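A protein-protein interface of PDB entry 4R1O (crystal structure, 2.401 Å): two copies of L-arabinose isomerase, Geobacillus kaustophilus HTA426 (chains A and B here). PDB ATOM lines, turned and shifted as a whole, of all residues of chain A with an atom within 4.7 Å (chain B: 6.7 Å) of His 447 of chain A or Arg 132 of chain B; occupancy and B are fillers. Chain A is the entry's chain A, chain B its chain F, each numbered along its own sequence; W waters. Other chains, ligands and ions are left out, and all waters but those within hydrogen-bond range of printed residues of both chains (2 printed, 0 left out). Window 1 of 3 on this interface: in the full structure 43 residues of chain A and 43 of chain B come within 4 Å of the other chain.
No position is printed for both chains.
His 447 of chain A touches just these residues of chain B: Phe 84 (3.7 Å), His 129 (3.3 Å), Arg 132 (3.96 Å) and Glu 133 (3.98 Å). Of the printed residues of chain A, Arg 132 of chain B touches Asp 333 (3.6 Å), Tyr 336 (2.9 Å), Ile 345 (3.99 Å), Ala 437 (3.7 Å), Trp 440 (3.4 Å), Gly 445 (3.5 Å) and His 447 (3.96 Å). Printed residues of chain B within 4 Å of Asp 333 of chain A: Ala 128, His 129 and Arg 132. Of the printed residues of chain A, His 105 of chain B touches Tyr 336 (2.6 Å) and Ala 437 (3.8 Å). Thr 449 of chain A touches none of the printed residues of chain B. His 448 of chain A touches none of the printed residues of chain B. The nearest residue of chain B that does not touch His 447 of chain A is Gly 130 of chain B (5.3 Å).
N of Val 191 of chain A sits at hydrogen-bond distance from OE1 of Glu 133 of chain B, 3.0 Å away. O of Asp 333 of chain A sits at hydrogen-bond distance from ND1 of His 129 of chain B, 2.7 Å away. The side-chain carboxylate (OD2) of Asp 333 of chain A is in salt-bridge range of the guanidinium group (NH1) of Arg 132 of chain B, 3.7 Å away. NE2 of His 105 of chain B is in hydrogen-bond range of OH of Tyr 336 of chain A (2.6 Å). OH of Tyr 336 of chain A sits at hydrogen-bond distance from NH1 of Arg 132 of chain B (2.9 Å).
OE2 of Glu 332 of chain A lies within hydrogen-bond range of ND1 of His 447 of chain A (3.0 Å). The backbone carbonyl oxygen of Trp 440 of chain A sits at hydrogen-bond distance from the backbone NH of Gly 445 of chain A (2.9 Å). The backbone carbonyl oxygen (O) of Ala 446 of chain A sits at hydrogen-bond distance from the indole nitrogen (NE1) of Trp 440 of chain A (3.0 Å). OD2 of Asp 131 of chain B lies within hydrogen-bond range of ND1 of His 105 of chain B, at 2.7 Å. O of Ala 128 of chain B is in hydrogen-bond range of NE of Arg 132 of chain B (2.9 Å).
Water W2 lies within hydrogen-bond range of OD1 of Asp 333 of chain A, NH2 of Arg 132 of chain B, O of Ala 446 of chain A and NE1 of Trp 440 of chain A. Water W1 lies within hydrogen-bond range of the backbone carbonyl oxygen of Gly 445 of chain A (2.8 Å) and the backbone carbonyl oxygen of Arg 132 of chain B (2.9 Å).
Along chain B the printed residues that touch a printed residue of chain A span positions 84 to 136. Of the 16 printed residues of chain A, 10 touch a printed residue of chain B. Hydrophobic or aromatic side chains of chain A within 4 Å of the printed part of chain B: Val 189, Val 191, Tyr 336, Ile 345, Ala 437, Trp 440 and His 447. Among the printed residues, 20 pairs touch across the chains. Among the printed residues, Asp or Glu carboxylates within 4 Å of a Lys or Arg side-chain nitrogen of the other chain: Asp 333 of chain A with Arg 132 of chain B (3.7 Å).
CG2 of Val 189 of chain A touches CE2 of Phe 84 of chain B, at 3.5 Å. OE2 of Glu 133 of chain B touches CA of Val 189 of chain A (3.7 Å). Phe 136 of chain B touches Val 191 of chain A (CD1 to CA, 3.4 Å). CG of His 129 of chain B touches OE2 of Glu 332 of chain A (3.3 Å). O of Asp 333 of chain A touches CB of Ala 128 of chain B (3.6 Å). CE1 of Tyr 336 of chain A touches CB of Ala 128 of chain B, 3.8 Å away. Gly 445 of chain A touches Arg 132 of chain B. Phe 84 of chain B touches His 447 of chain A (CE1 to CE1, 3.7 Å). His 447 of chain A touches His 129 of chain B (CB to CB, 3.3 Å). CD2 of His 447 of chain A touches CB of Glu 133 of chain B (3.98 Å).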
ATOM      1  N   VAL A 189     -29.957  -4.498  -2.269  1.00  0.00           N
ATOM      2  CA  VAL A 189     -28.786  -5.351  -2.004  1.00  0.00           C
ATOM      3  C   VAL A 189     -28.765  -5.880  -0.558  1.00  0.00           C
ATOM      4  O   VAL A 189     -29.077  -5.143   0.380  1.00  0.00           O
ATOM      5  CB  VAL A 189     -27.447  -4.630  -2.366  1.00  0.00           C
ATOM      6  CG1 VAL A 189     -26.234  -5.434  -1.907  1.00  0.00           C
ATOM      7  CG2 VAL A 189     -27.364  -4.401  -3.851  1.00  0.00           C
ATOM      8  N   VAL A 191     -26.116  -8.289   1.125  1.00  0.00           N
ATOM      9  CA  VAL A 191     -24.915  -8.627   1.886  1.00  0.00           C
ATOM     10  C   VAL A 191     -24.270  -7.395   2.505  1.00  0.00           C
ATOM     11  O   VAL A 191     -23.630  -7.496   3.544  1.00  0.00           O
ATOM     12  CB  VAL A 191     -23.890  -9.430   1.037  1.00  0.00           C
ATOM     13  CG1 VAL A 191     -23.191  -8.534   0.055  1.00  0.00           C
ATOM     14  CG2 VAL A 191     -22.883 -10.157   1.932  1.00  0.00           C
ATOM     15  N   THR A 192     -24.463  -6.233   1.881  1.00  0.00           N
ATOM     16  CA  THR A 192     -23.879  -4.989   2.383  1.00  0.00           C
ATOM     17  C   THR A 192     -24.755  -4.377   3.486  1.00  0.00           C
ATOM     18  O   THR A 192     -24.387  -3.399   4.135  1.00  0.00           O
ATOM     19  CB  THR A 192     -23.692  -3.962   1.250  1.00  0.00           C
ATOM     20  OG1 THR A 192     -24.959  -3.696   0.645  1.00  0.00           O
ATOM     21  CG2 THR A 192     -22.746  -4.490   0.184  1.00  0.00           C
ATOM     22  N   GLU A 307     -20.790   1.102  -2.927  1.00  0.00           N
ATOM     23  CA  GLU A 307     -22.232   0.962  -2.704  1.00  0.00           C
ATOM     24  C   GLU A 307     -22.666   0.932  -1.228  1.00  0.00           C
ATOM     25  O   GLU A 307     -23.386   0.029  -0.812  1.00  0.00           O
ATOM     26  CB  GLU A 307     -22.755  -0.294  -3.411  1.00  0.00           C
ATOM     27  CG  GLU A 307     -22.587  -0.276  -4.916  1.00  0.00           C
ATOM     28  CD  GLU A 307     -21.426  -1.138  -5.390  1.00  0.00           C
ATOM     29  OE1 GLU A 307     -21.466  -2.385  -5.195  1.00  0.00           O
ATOM     30  OE2 GLU A 307     -20.475  -0.565  -5.967  1.00  0.00           O
ATOM     31  N   MET A 331     -11.981  -4.917  -2.975  1.00  0.00           N
ATOM     32  CA  MET A 331     -11.877  -5.847  -4.086  1.00  0.00           C
ATOM     33  C   MET A 331     -13.213  -6.539  -4.297  1.00  0.00           C
ATOM     34  O   MET A 331     -13.977  -6.734  -3.353  1.00  0.00           O
ATOM     35  CB  MET A 331     -10.786  -6.893  -3.798  1.00  0.00           C
ATOM     36  CG  MET A 331     -10.497  -7.853  -4.959  1.00  0.00           C
ATOM     37  SD  MET A 331     -10.122  -6.960  -6.494  1.00  0.00           S
ATOM     38  CE  MET A 331      -8.600  -6.125  -6.067  1.00  0.00           C
ATOM     39  N   GLU A 332     -13.494  -6.904  -5.538  1.00  0.00           N
ATOM     40  CA  GLU A 332     -14.715  -7.622  -5.871  1.00  0.00           C
ATOM     41  C   GLU A 332     -14.423  -8.607  -7.002  1.00  0.00           C
ATOM     42  O   GLU A 332     -13.760  -8.247  -7.972  1.00  0.00           O
ATOM     43  CB  GLU A 332     -15.814  -6.636  -6.283  1.00  0.00           C
ATOM     44  CG  GLU A 332     -17.087  -7.303  -6.779  1.00  0.00           C
ATOM     45  CD  GLU A 332     -18.152  -6.296  -7.177  1.00  0.00           C
ATOM     46  OE1 GLU A 332     -17.790  -5.235  -7.715  1.00  0.00           O
ATOM     47  OE2 GLU A 332     -19.354  -6.557  -6.953  1.00  0.00           O
ATOM     48  N   ASP A 333     -14.893  -9.848  -6.877  1.00  0.00           N
ATOM     49  CA  ASP A 333     -14.693 -10.837  -7.946  1.00  0.00           C
ATOM     50  C   ASP A 333     -15.517 -10.435  -9.155  1.00  0.00           C
ATOM     51  O   ASP A 333     -16.748 -10.302  -9.059  1.00  0.00           O
ATOM     52  CB  ASP A 333     -15.116 -12.233  -7.505  1.00  0.00           C
ATOM     53  CG  ASP A 333     -14.551 -12.615  -6.158  1.00  0.00           C
ATOM     54  OD1 ASP A 333     -14.949 -11.985  -5.140  1.00  0.00           O
ATOM     55  OD2 ASP A 333     -13.733 -13.562  -6.117  1.00  0.00           O
ATOM     56  N   TYR A 336     -14.596 -14.929 -14.330  1.00  0.00           N
ATOM     57  CA  TYR A 336     -13.754 -16.119 -14.195  1.00  0.00           C
ATOM     58  C   TYR A 336     -13.055 -16.509 -15.493  1.00  0.00           C
ATOM     59  O   TYR A 336     -13.544 -16.231 -16.581  1.00  0.00           O
ATOM     60  CB  TYR A 336     -14.599 -17.317 -13.763  1.00  0.00           C
ATOM     61  CG  TYR A 336     -15.127 -17.269 -12.351  1.00  0.00           C
ATOM     62  CD1 TYR A 336     -14.476 -16.549 -11.357  1.00  0.00           C
ATOM     63  CD2 TYR A 336     -16.279 -17.960 -12.009  1.00  0.00           C
ATOM     64  CE1 TYR A 336     -14.975 -16.526 -10.055  1.00  0.00           C
ATOM     65  CE2 TYR A 336     -16.772 -17.938 -10.736  1.00  0.00           C
ATOM     66  CZ  TYR A 336     -16.120 -17.228  -9.760  1.00  0.00           C
ATOM     67  OH  TYR A 336     -16.649 -17.215  -8.494  1.00  0.00           O
ATOM     68  N   ILE A 345      -9.502 -16.129 -11.127  1.00  0.00           N
ATOM     69  CA  ILE A 345     -10.499 -15.102 -10.881  1.00  0.00           C
ATOM     70  C   ILE A 345      -9.895 -13.751 -11.230  1.00  0.00           C
ATOM     71  O   ILE A 345      -8.750 -13.463 -10.878  1.00  0.00           O
ATOM     72  CB  ILE A 345     -10.925 -15.092  -9.401  1.00  0.00           C
ATOM     73  CG1 ILE A 345     -11.399 -16.481  -8.972  1.00  0.00           C
ATOM     74  CG2 ILE A 345     -12.009 -14.046  -9.141  1.00  0.00           C
ATOM     75  CD1 ILE A 345     -11.882 -16.540  -7.519  1.00  0.00           C
ATOM     76  N   ALA A 437     -14.856 -21.362  -4.162  1.00  0.00           N
ATOM     77  CA  ALA A 437     -16.121 -20.687  -4.402  1.00  0.00           C
ATOM     78  C   ALA A 437     -17.297 -21.447  -3.779  1.00  0.00           C
ATOM     79  O   ALA A 437     -18.229 -20.824  -3.270  1.00  0.00           O
ATOM     80  CB  ALA A 437     -16.349 -20.434  -5.876  1.00  0.00           C
ATOM     81  N   TRP A 440     -16.957 -20.757  -0.024  1.00  0.00           N
ATOM     82  CA  TRP A 440     -17.300 -19.353   0.163  1.00  0.00           C
ATOM     83  C   TRP A 440     -18.816 -19.119   0.120  1.00  0.00           C
ATOM     84  O   TRP A 440     -19.375 -18.477   1.000  1.00  0.00           O
ATOM     85  CB  TRP A 440     -16.614 -18.522  -0.905  1.00  0.00           C
ATOM     86  CG  TRP A 440     -16.693 -17.059  -0.700  1.00  0.00           C
ATOM     87  CD1 TRP A 440     -17.718 -16.230  -1.062  1.00  0.00           C
ATOM     88  CD2 TRP A 440     -15.686 -16.228  -0.126  1.00  0.00           C
ATOM     89  NE1 TRP A 440     -17.411 -14.935  -0.739  1.00  0.00           N
ATOM     90  CE2 TRP A 440     -16.171 -14.906  -0.155  1.00  0.00           C
ATOM     91  CE3 TRP A 440     -14.425 -16.475   0.420  1.00  0.00           C
ATOM     92  CZ2 TRP A 440     -15.440 -13.835   0.340  1.00  0.00           C
ATOM     93  CZ3 TRP A 440     -13.702 -15.415   0.905  1.00  0.00           C
ATOM     94  CH2 TRP A 440     -14.212 -14.109   0.870  1.00  0.00           C
ATOM     95  N   GLY A 445     -20.162 -15.843   2.018  1.00  0.00           N
ATOM     96  CA  GLY A 445     -19.247 -14.730   1.837  1.00  0.00           C
ATOM     97  C   GLY A 445     -19.700 -13.700   0.817  1.00  0.00           C
ATOM     98  O   GLY A 445     -20.312 -14.034  -0.208  1.00  0.00           O
ATOM     99  N   ALA A 446     -19.395 -12.440   1.098  1.00  0.00           N
ATOM    100  CA  ALA A 446     -19.788 -11.348   0.219  1.00  0.00           C
ATOM    101  C   ALA A 446     -19.088 -11.394  -1.136  1.00  0.00           C
ATOM    102  O   ALA A 446     -18.092 -12.109  -1.328  1.00  0.00           O
ATOM    103  CB  ALA A 446     -19.536  -9.997   0.894  1.00  0.00           C
ATOM    104  N   HIS A 447     -19.634 -10.633  -2.075  1.00  0.00           N
ATOM    105  CA  HIS A 447     -18.948 -10.306  -3.318  1.00  0.00           C
ATOM    106  C   HIS A 447     -17.870  -9.237  -3.084  1.00  0.00           C
ATOM    107  O   HIS A 447     -16.850  -9.210  -3.771  1.00  0.00           O
ATOM    108  CB  HIS A 447     -19.951  -9.803  -4.354  1.00  0.00           C
ATOM    109  CG  HIS A 447     -20.796  -8.665  -3.880  1.00  0.00           C
ATOM    110  ND1 HIS A 447     -20.834  -7.447  -4.527  1.00  0.00           N
ATOM    111  CD2 HIS A 447     -21.645  -8.560  -2.831  1.00  0.00           C
ATOM    112  CE1 HIS A 447     -21.661  -6.638  -3.888  1.00  0.00           C
ATOM    113  NE2 HIS A 447     -22.164  -7.289  -2.854  1.00  0.00           N
ATOM    114  N   HIS A 448     -18.112  -8.344  -2.124  1.00  0.00           N
ATOM    115  CA  HIS A 448     -17.120  -7.346  -1.732  1.00  0.00           C
ATOM    116  C   HIS A 448     -16.152  -7.956  -0.726  1.00  0.00           C
ATOM    117  O   HIS A 448     -16.567  -8.685   0.172  1.00  0.00           O
ATOM    118  CB  HIS A 448     -17.800  -6.112  -1.119  1.00  0.00           C
ATOM    119  CG  HIS A 448     -18.499  -5.249  -2.125  1.00  0.00           C
ATOM    120  ND1 HIS A 448     -19.171  -4.100  -1.779  1.00  0.00           N
ATOM    121  CD2 HIS A 448     -18.628  -5.368  -3.468  1.00  0.00           C
ATOM    122  CE1 HIS A 448     -19.698  -3.553  -2.860  1.00  0.00           C
ATOM    123  NE2 HIS A 448     -19.379  -4.304  -3.900  1.00  0.00           N
ATOM    124  N   THR A 449     -14.862  -7.666  -0.881  1.00  0.00           N
ATOM    125  CA  THR A 449     -13.853  -8.201   0.024  1.00  0.00           C
ATOM    126  C   THR A 449     -12.737  -7.204   0.231  1.00  0.00           C
ATOM    127  O   THR A 449     -12.655  -6.186  -0.455  1.00  0.00           O
ATOM    128  CB  THR A 449     -13.142  -9.467  -0.529  1.00  0.00           C
ATOM    129  OG1 THR A 449     -12.243  -9.080  -1.574  1.00  0.00           O
ATOM    130  CG2 THR A 449     -14.125 -10.512  -1.059  1.00  0.00           C
ATOM    131  N   MET B  81     -27.294 -16.668 -10.992  1.00  0.00           N
ATOM    132  CA  MET B  81     -27.257 -15.225 -11.197  1.00  0.00           C
ATOM    133  C   MET B  81     -26.304 -14.914 -12.344  1.00  0.00           C
ATOM    134  O   MET B  81     -25.092 -14.932 -12.162  1.00  0.00           O
ATOM    135  CB  MET B  81     -26.812 -14.486  -9.922  1.00  0.00           C
ATOM    136  CG  MET B  81     -27.560 -14.875  -8.648  1.00  0.00           C
ATOM    137  SD  MET B  81     -29.380 -14.843  -8.734  1.00  0.00           S
ATOM    138  CE  MET B  81     -29.742 -16.605  -8.603  1.00  0.00           C
ATOM    139  N   PHE B  84     -25.275  -9.459 -11.411  1.00  0.00           N
ATOM    140  CA  PHE B  84     -25.669  -9.031 -10.095  1.00  0.00           C
ATOM    141  C   PHE B  84     -27.187  -8.957 -10.075  1.00  0.00           C
ATOM    142  O   PHE B  84     -27.809  -8.413 -10.986  1.00  0.00           O
ATOM    143  CB  PHE B  84     -25.050  -7.667  -9.771  1.00  0.00           C
ATOM    144  CG  PHE B  84     -25.039  -7.341  -8.310  1.00  0.00           C
ATOM    145  CD1 PHE B  84     -24.470  -8.217  -7.395  1.00  0.00           C
ATOM    146  CD2 PHE B  84     -25.586  -6.162  -7.844  1.00  0.00           C
ATOM    147  CE1 PHE B  84     -24.449  -7.911  -6.041  1.00  0.00           C
ATOM    148  CE2 PHE B  84     -25.563  -5.856  -6.486  1.00  0.00           C
ATOM    149  CZ  PHE B  84     -24.998  -6.733  -5.588  1.00  0.00           C
ATOM    150  N   HIS B 103     -28.146 -24.288  -6.361  1.00  0.00           N
ATOM    151  CA  HIS B 103     -27.577 -23.042  -6.818  1.00  0.00           C
ATOM    152  C   HIS B 103     -26.433 -23.421  -7.729  1.00  0.00           C
ATOM    153  O   HIS B 103     -25.454 -24.012  -7.270  1.00  0.00           O
ATOM    154  CB  HIS B 103     -27.089 -22.225  -5.625  1.00  0.00           C
ATOM    155  CG  HIS B 103     -26.352 -20.981  -5.999  1.00  0.00           C
ATOM    156  ND1 HIS B 103     -25.622 -20.253  -5.084  1.00  0.00           N
ATOM    157  CD2 HIS B 103     -26.236 -20.329  -7.181  1.00  0.00           C
ATOM    158  CE1 HIS B 103     -25.076 -19.213  -5.691  1.00  0.00           C
ATOM    159  NE2 HIS B 103     -25.430 -19.237  -6.964  1.00  0.00           N
ATOM    160  N   HIS B 105     -23.380 -22.232  -9.777  1.00  0.00           N
ATOM    161  CA  HIS B 105     -22.486 -21.082  -9.875  1.00  0.00           C
ATOM    162  C   HIS B 105     -21.606 -21.282 -11.109  1.00  0.00           C
ATOM    163  O   HIS B 105     -20.658 -22.067 -11.093  1.00  0.00           O
ATOM    164  CB  HIS B 105     -21.661 -20.938  -8.583  1.00  0.00           C
ATOM    165  CG  HIS B 105     -20.657 -19.830  -8.620  1.00  0.00           C
ATOM    166  ND1 HIS B 105     -20.877 -18.645  -9.291  1.00  0.00           N
ATOM    167  CD2 HIS B 105     -19.422 -19.729  -8.071  1.00  0.00           C
ATOM    168  CE1 HIS B 105     -19.818 -17.863  -9.158  1.00  0.00           C
ATOM    169  NE2 HIS B 105     -18.923 -18.495  -8.417  1.00  0.00           N
ATOM    170  N   SER B 127     -21.190 -13.297 -12.860  1.00  0.00           N
ATOM    171  CA  SER B 127     -21.667 -14.313 -11.927  1.00  0.00           C
ATOM    172  C   SER B 127     -20.691 -14.443 -10.780  1.00  0.00           C
ATOM    173  O   SER B 127     -21.071 -14.829  -9.671  1.00  0.00           O
ATOM    174  CB  SER B 127     -21.763 -15.676 -12.602  1.00  0.00           C
ATOM    175  OG  SER B 127     -22.883 -15.757 -13.442  1.00  0.00           O
ATOM    176  N   ALA B 128     -19.429 -14.135 -11.079  1.00  0.00           N
ATOM    177  CA  ALA B 128     -18.356 -14.153 -10.095  1.00  0.00           C
ATOM    178  C   ALA B 128     -18.791 -13.451  -8.817  1.00  0.00           C
ATOM    179  O   ALA B 128     -18.445 -13.885  -7.733  1.00  0.00           O
ATOM    180  CB  ALA B 128     -17.110 -13.488 -10.661  1.00  0.00           C
ATOM    181  N   HIS B 129     -19.549 -12.366  -8.942  1.00  0.00           N
ATOM    182  CA  HIS B 129     -20.064 -11.723  -7.753  1.00  0.00           C
ATOM    183  C   HIS B 129     -21.574 -11.824  -7.565  1.00  0.00           C
ATOM    184  O   HIS B 129     -22.041 -11.855  -6.424  1.00  0.00           O
ATOM    185  CB  HIS B 129     -19.537 -10.296  -7.586  1.00  0.00           C
ATOM    186  CG  HIS B 129     -19.899  -9.354  -8.686  1.00  0.00           C
ATOM    187  ND1 HIS B 129     -18.998  -8.971  -9.657  1.00  0.00           N
ATOM    188  CD2 HIS B 129     -21.039  -8.668  -8.933  1.00  0.00           C
ATOM    189  CE1 HIS B 129     -19.578  -8.105 -10.470  1.00  0.00           C
ATOM    190  NE2 HIS B 129     -20.816  -7.904 -10.052  1.00  0.00           N
ATOM    191  N   GLY B 130     -22.326 -11.899  -8.665  1.00  0.00           N
ATOM    192  CA  GLY B 130     -23.764 -12.106  -8.590  1.00  0.00           C
ATOM    193  C   GLY B 130     -24.181 -13.309  -7.751  1.00  0.00           C
ATOM    194  O   GLY B 130     -25.103 -13.230  -6.933  1.00  0.00           O
ATOM    195  N   ASP B 131     -23.479 -14.423  -7.934  1.00  0.00           N
ATOM    196  CA  ASP B 131     -23.752 -15.643  -7.179  1.00  0.00           C
ATOM    197  C   ASP B 131     -23.268 -15.610  -5.737  1.00  0.00           C
ATOM    198  O   ASP B 131     -23.767 -16.372  -4.906  1.00  0.00           O
ATOM    199  CB  ASP B 131     -23.135 -16.854  -7.872  1.00  0.00           C
ATOM    200  CG  ASP B 131     -23.869 -17.240  -9.137  1.00  0.00           C
ATOM    201  OD1 ASP B 131     -25.117 -17.187  -9.130  1.00  0.00           O
ATOM    202  OD2 ASP B 131     -23.199 -17.605 -10.135  1.00  0.00           O
ATOM    203  N   ARG B 132     -22.274 -14.778  -5.437  1.00  0.00           N
ATOM    204  CA  ARG B 132     -21.827 -14.628  -4.051  1.00  0.00           C
ATOM    205  C   ARG B 132     -22.874 -13.849  -3.223  1.00  0.00           C
ATOM    206  O   ARG B 132     -23.245 -14.266  -2.115  1.00  0.00           O
ATOM    207  CB  ARG B 132     -20.421 -14.013  -3.978  1.00  0.00           C
ATOM    208  CG  ARG B 132     -19.380 -14.917  -4.636  1.00  0.00           C
ATOM    209  CD  ARG B 132     -17.956 -14.339  -4.747  1.00  0.00           C
ATOM    210  NE  ARG B 132     -17.147 -15.262  -5.545  1.00  0.00           N
ATOM    211  CZ  ARG B 132     -16.148 -16.007  -5.074  1.00  0.00           C
ATOM    212  NH1 ARG B 132     -15.515 -16.846  -5.889  1.00  0.00           N
ATOM    213  NH2 ARG B 132     -15.773 -15.918  -3.799  1.00  0.00           N
ATOM    214  N   GLU B 133     -23.380 -12.748  -3.778  1.00  0.00           N
ATOM    215  CA  GLU B 133     -24.457 -12.001  -3.128  1.00  0.00           C
ATOM    216  C   GLU B 133     -25.676 -12.914  -2.937  1.00  0.00           C
ATOM    217  O   GLU B 133     -26.295 -12.936  -1.874  1.00  0.00           O
ATOM    218  CB  GLU B 133     -24.798 -10.728  -3.919  1.00  0.00           C
ATOM    219  CG  GLU B 133     -26.251 -10.276  -3.829  1.00  0.00           C
ATOM    220  CD  GLU B 133     -26.595  -9.429  -2.589  1.00  0.00           C
ATOM    221  OE1 GLU B 133     -25.829  -9.407  -1.590  1.00  0.00           O
ATOM    222  OE2 GLU B 133     -27.665  -8.778  -2.627  1.00  0.00           O
ATOM    223  N   TYR B 134     -25.989 -13.708  -3.954  1.00  0.00           N
ATOM    224  CA  TYR B 134     -27.058 -14.690  -3.822  1.00  0.00           C
ATOM    225  C   TYR B 134     -26.695 -15.782  -2.824  1.00  0.00           C
ATOM    226  O   TYR B 134     -27.566 -16.313  -2.147  1.00  0.00           O
ATOM    227  CB  TYR B 134     -27.374 -15.313  -5.170  1.00  0.00           C
ATOM    228  CG  TYR B 134     -28.463 -16.352  -5.118  1.00  0.00           C
ATOM    229  CD1 TYR B 134     -29.794 -15.981  -4.959  1.00  0.00           C
ATOM    230  CD2 TYR B 134     -28.166 -17.705  -5.254  1.00  0.00           C
ATOM    231  CE1 TYR B 134     -30.792 -16.923  -4.910  1.00  0.00           C
ATOM    232  CE2 TYR B 134     -29.161 -18.653  -5.218  1.00  0.00           C
ATOM    233  CZ  TYR B 134     -30.473 -18.256  -5.050  1.00  0.00           C
ATOM    234  OH  TYR B 134     -31.469 -19.203  -5.017  1.00  0.00           O
ATOM    235  N   GLY B 135     -25.409 -16.117  -2.751  1.00  0.00           N
ATOM    236  CA  GLY B 135     -24.919 -17.086  -1.791  1.00  0.00           C
ATOM    237  C   GLY B 135     -25.145 -16.616  -0.362  1.00  0.00           C
ATOM    238  O   GLY B 135     -25.529 -17.400   0.497  1.00  0.00           O
ATOM    239  N   PHE B 136     -24.921 -15.330  -0.113  1.00  0.00           N
ATOM    240  CA  PHE B 136     -25.162 -14.756   1.208  1.00  0.00           C
ATOM    241  C   PHE B 136     -26.611 -14.863   1.689  1.00  0.00           C
ATOM    242  O   PHE B 136     -26.851 -15.271   2.823  1.00  0.00           O
ATOM    243  CB  PHE B 136     -24.771 -13.287   1.271  1.00  0.00           C
ATOM    244  CG  PHE B 136     -25.315 -12.603   2.490  1.00  0.00           C
ATOM    245  CD1 PHE B 136     -26.368 -11.709   2.393  1.00  0.00           C
ATOM    246  CD2 PHE B 136     -24.819 -12.918   3.751  1.00  0.00           C
ATOM    247  CE1 PHE B 136     -26.882 -11.119   3.528  1.00  0.00           C
ATOM    248  CE2 PHE B 136     -25.331 -12.322   4.879  1.00  0.00           C
ATOM    249  CZ  PHE B 136     -26.363 -11.421   4.770  1.00  0.00           C
ATOM    250  N   ILE B 137     -27.575 -14.468   0.853  1.00  0.00           N
ATOM    251  CA  ILE B 137     -28.969 -14.532   1.280  1.00  0.00           C
ATOM    252  C   ILE B 137     -29.397 -15.973   1.588  1.00  0.00           C
ATOM    253  O   ILE B 137     -30.173 -16.213   2.515  1.00  0.00           O
ATOM    254  CB  ILE B 137     -29.945 -13.818   0.293  1.00  0.00           C
ATOM    255  CG1 ILE B 137     -31.184 -13.327   1.047  1.00  0.00           C
ATOM    256  CG2 ILE B 137     -30.350 -14.725  -0.874  1.00  0.00           C
ATOM    257  CD1 ILE B 137     -30.858 -12.577   2.330  1.00  0.00           C
HETATM  258  O   HOH W   1     -21.617 -16.374  -0.982  1.00  0.00           O
HETATM  259  O   HOH W   2     -15.563 -13.023  -2.882  1.00  0.00           O
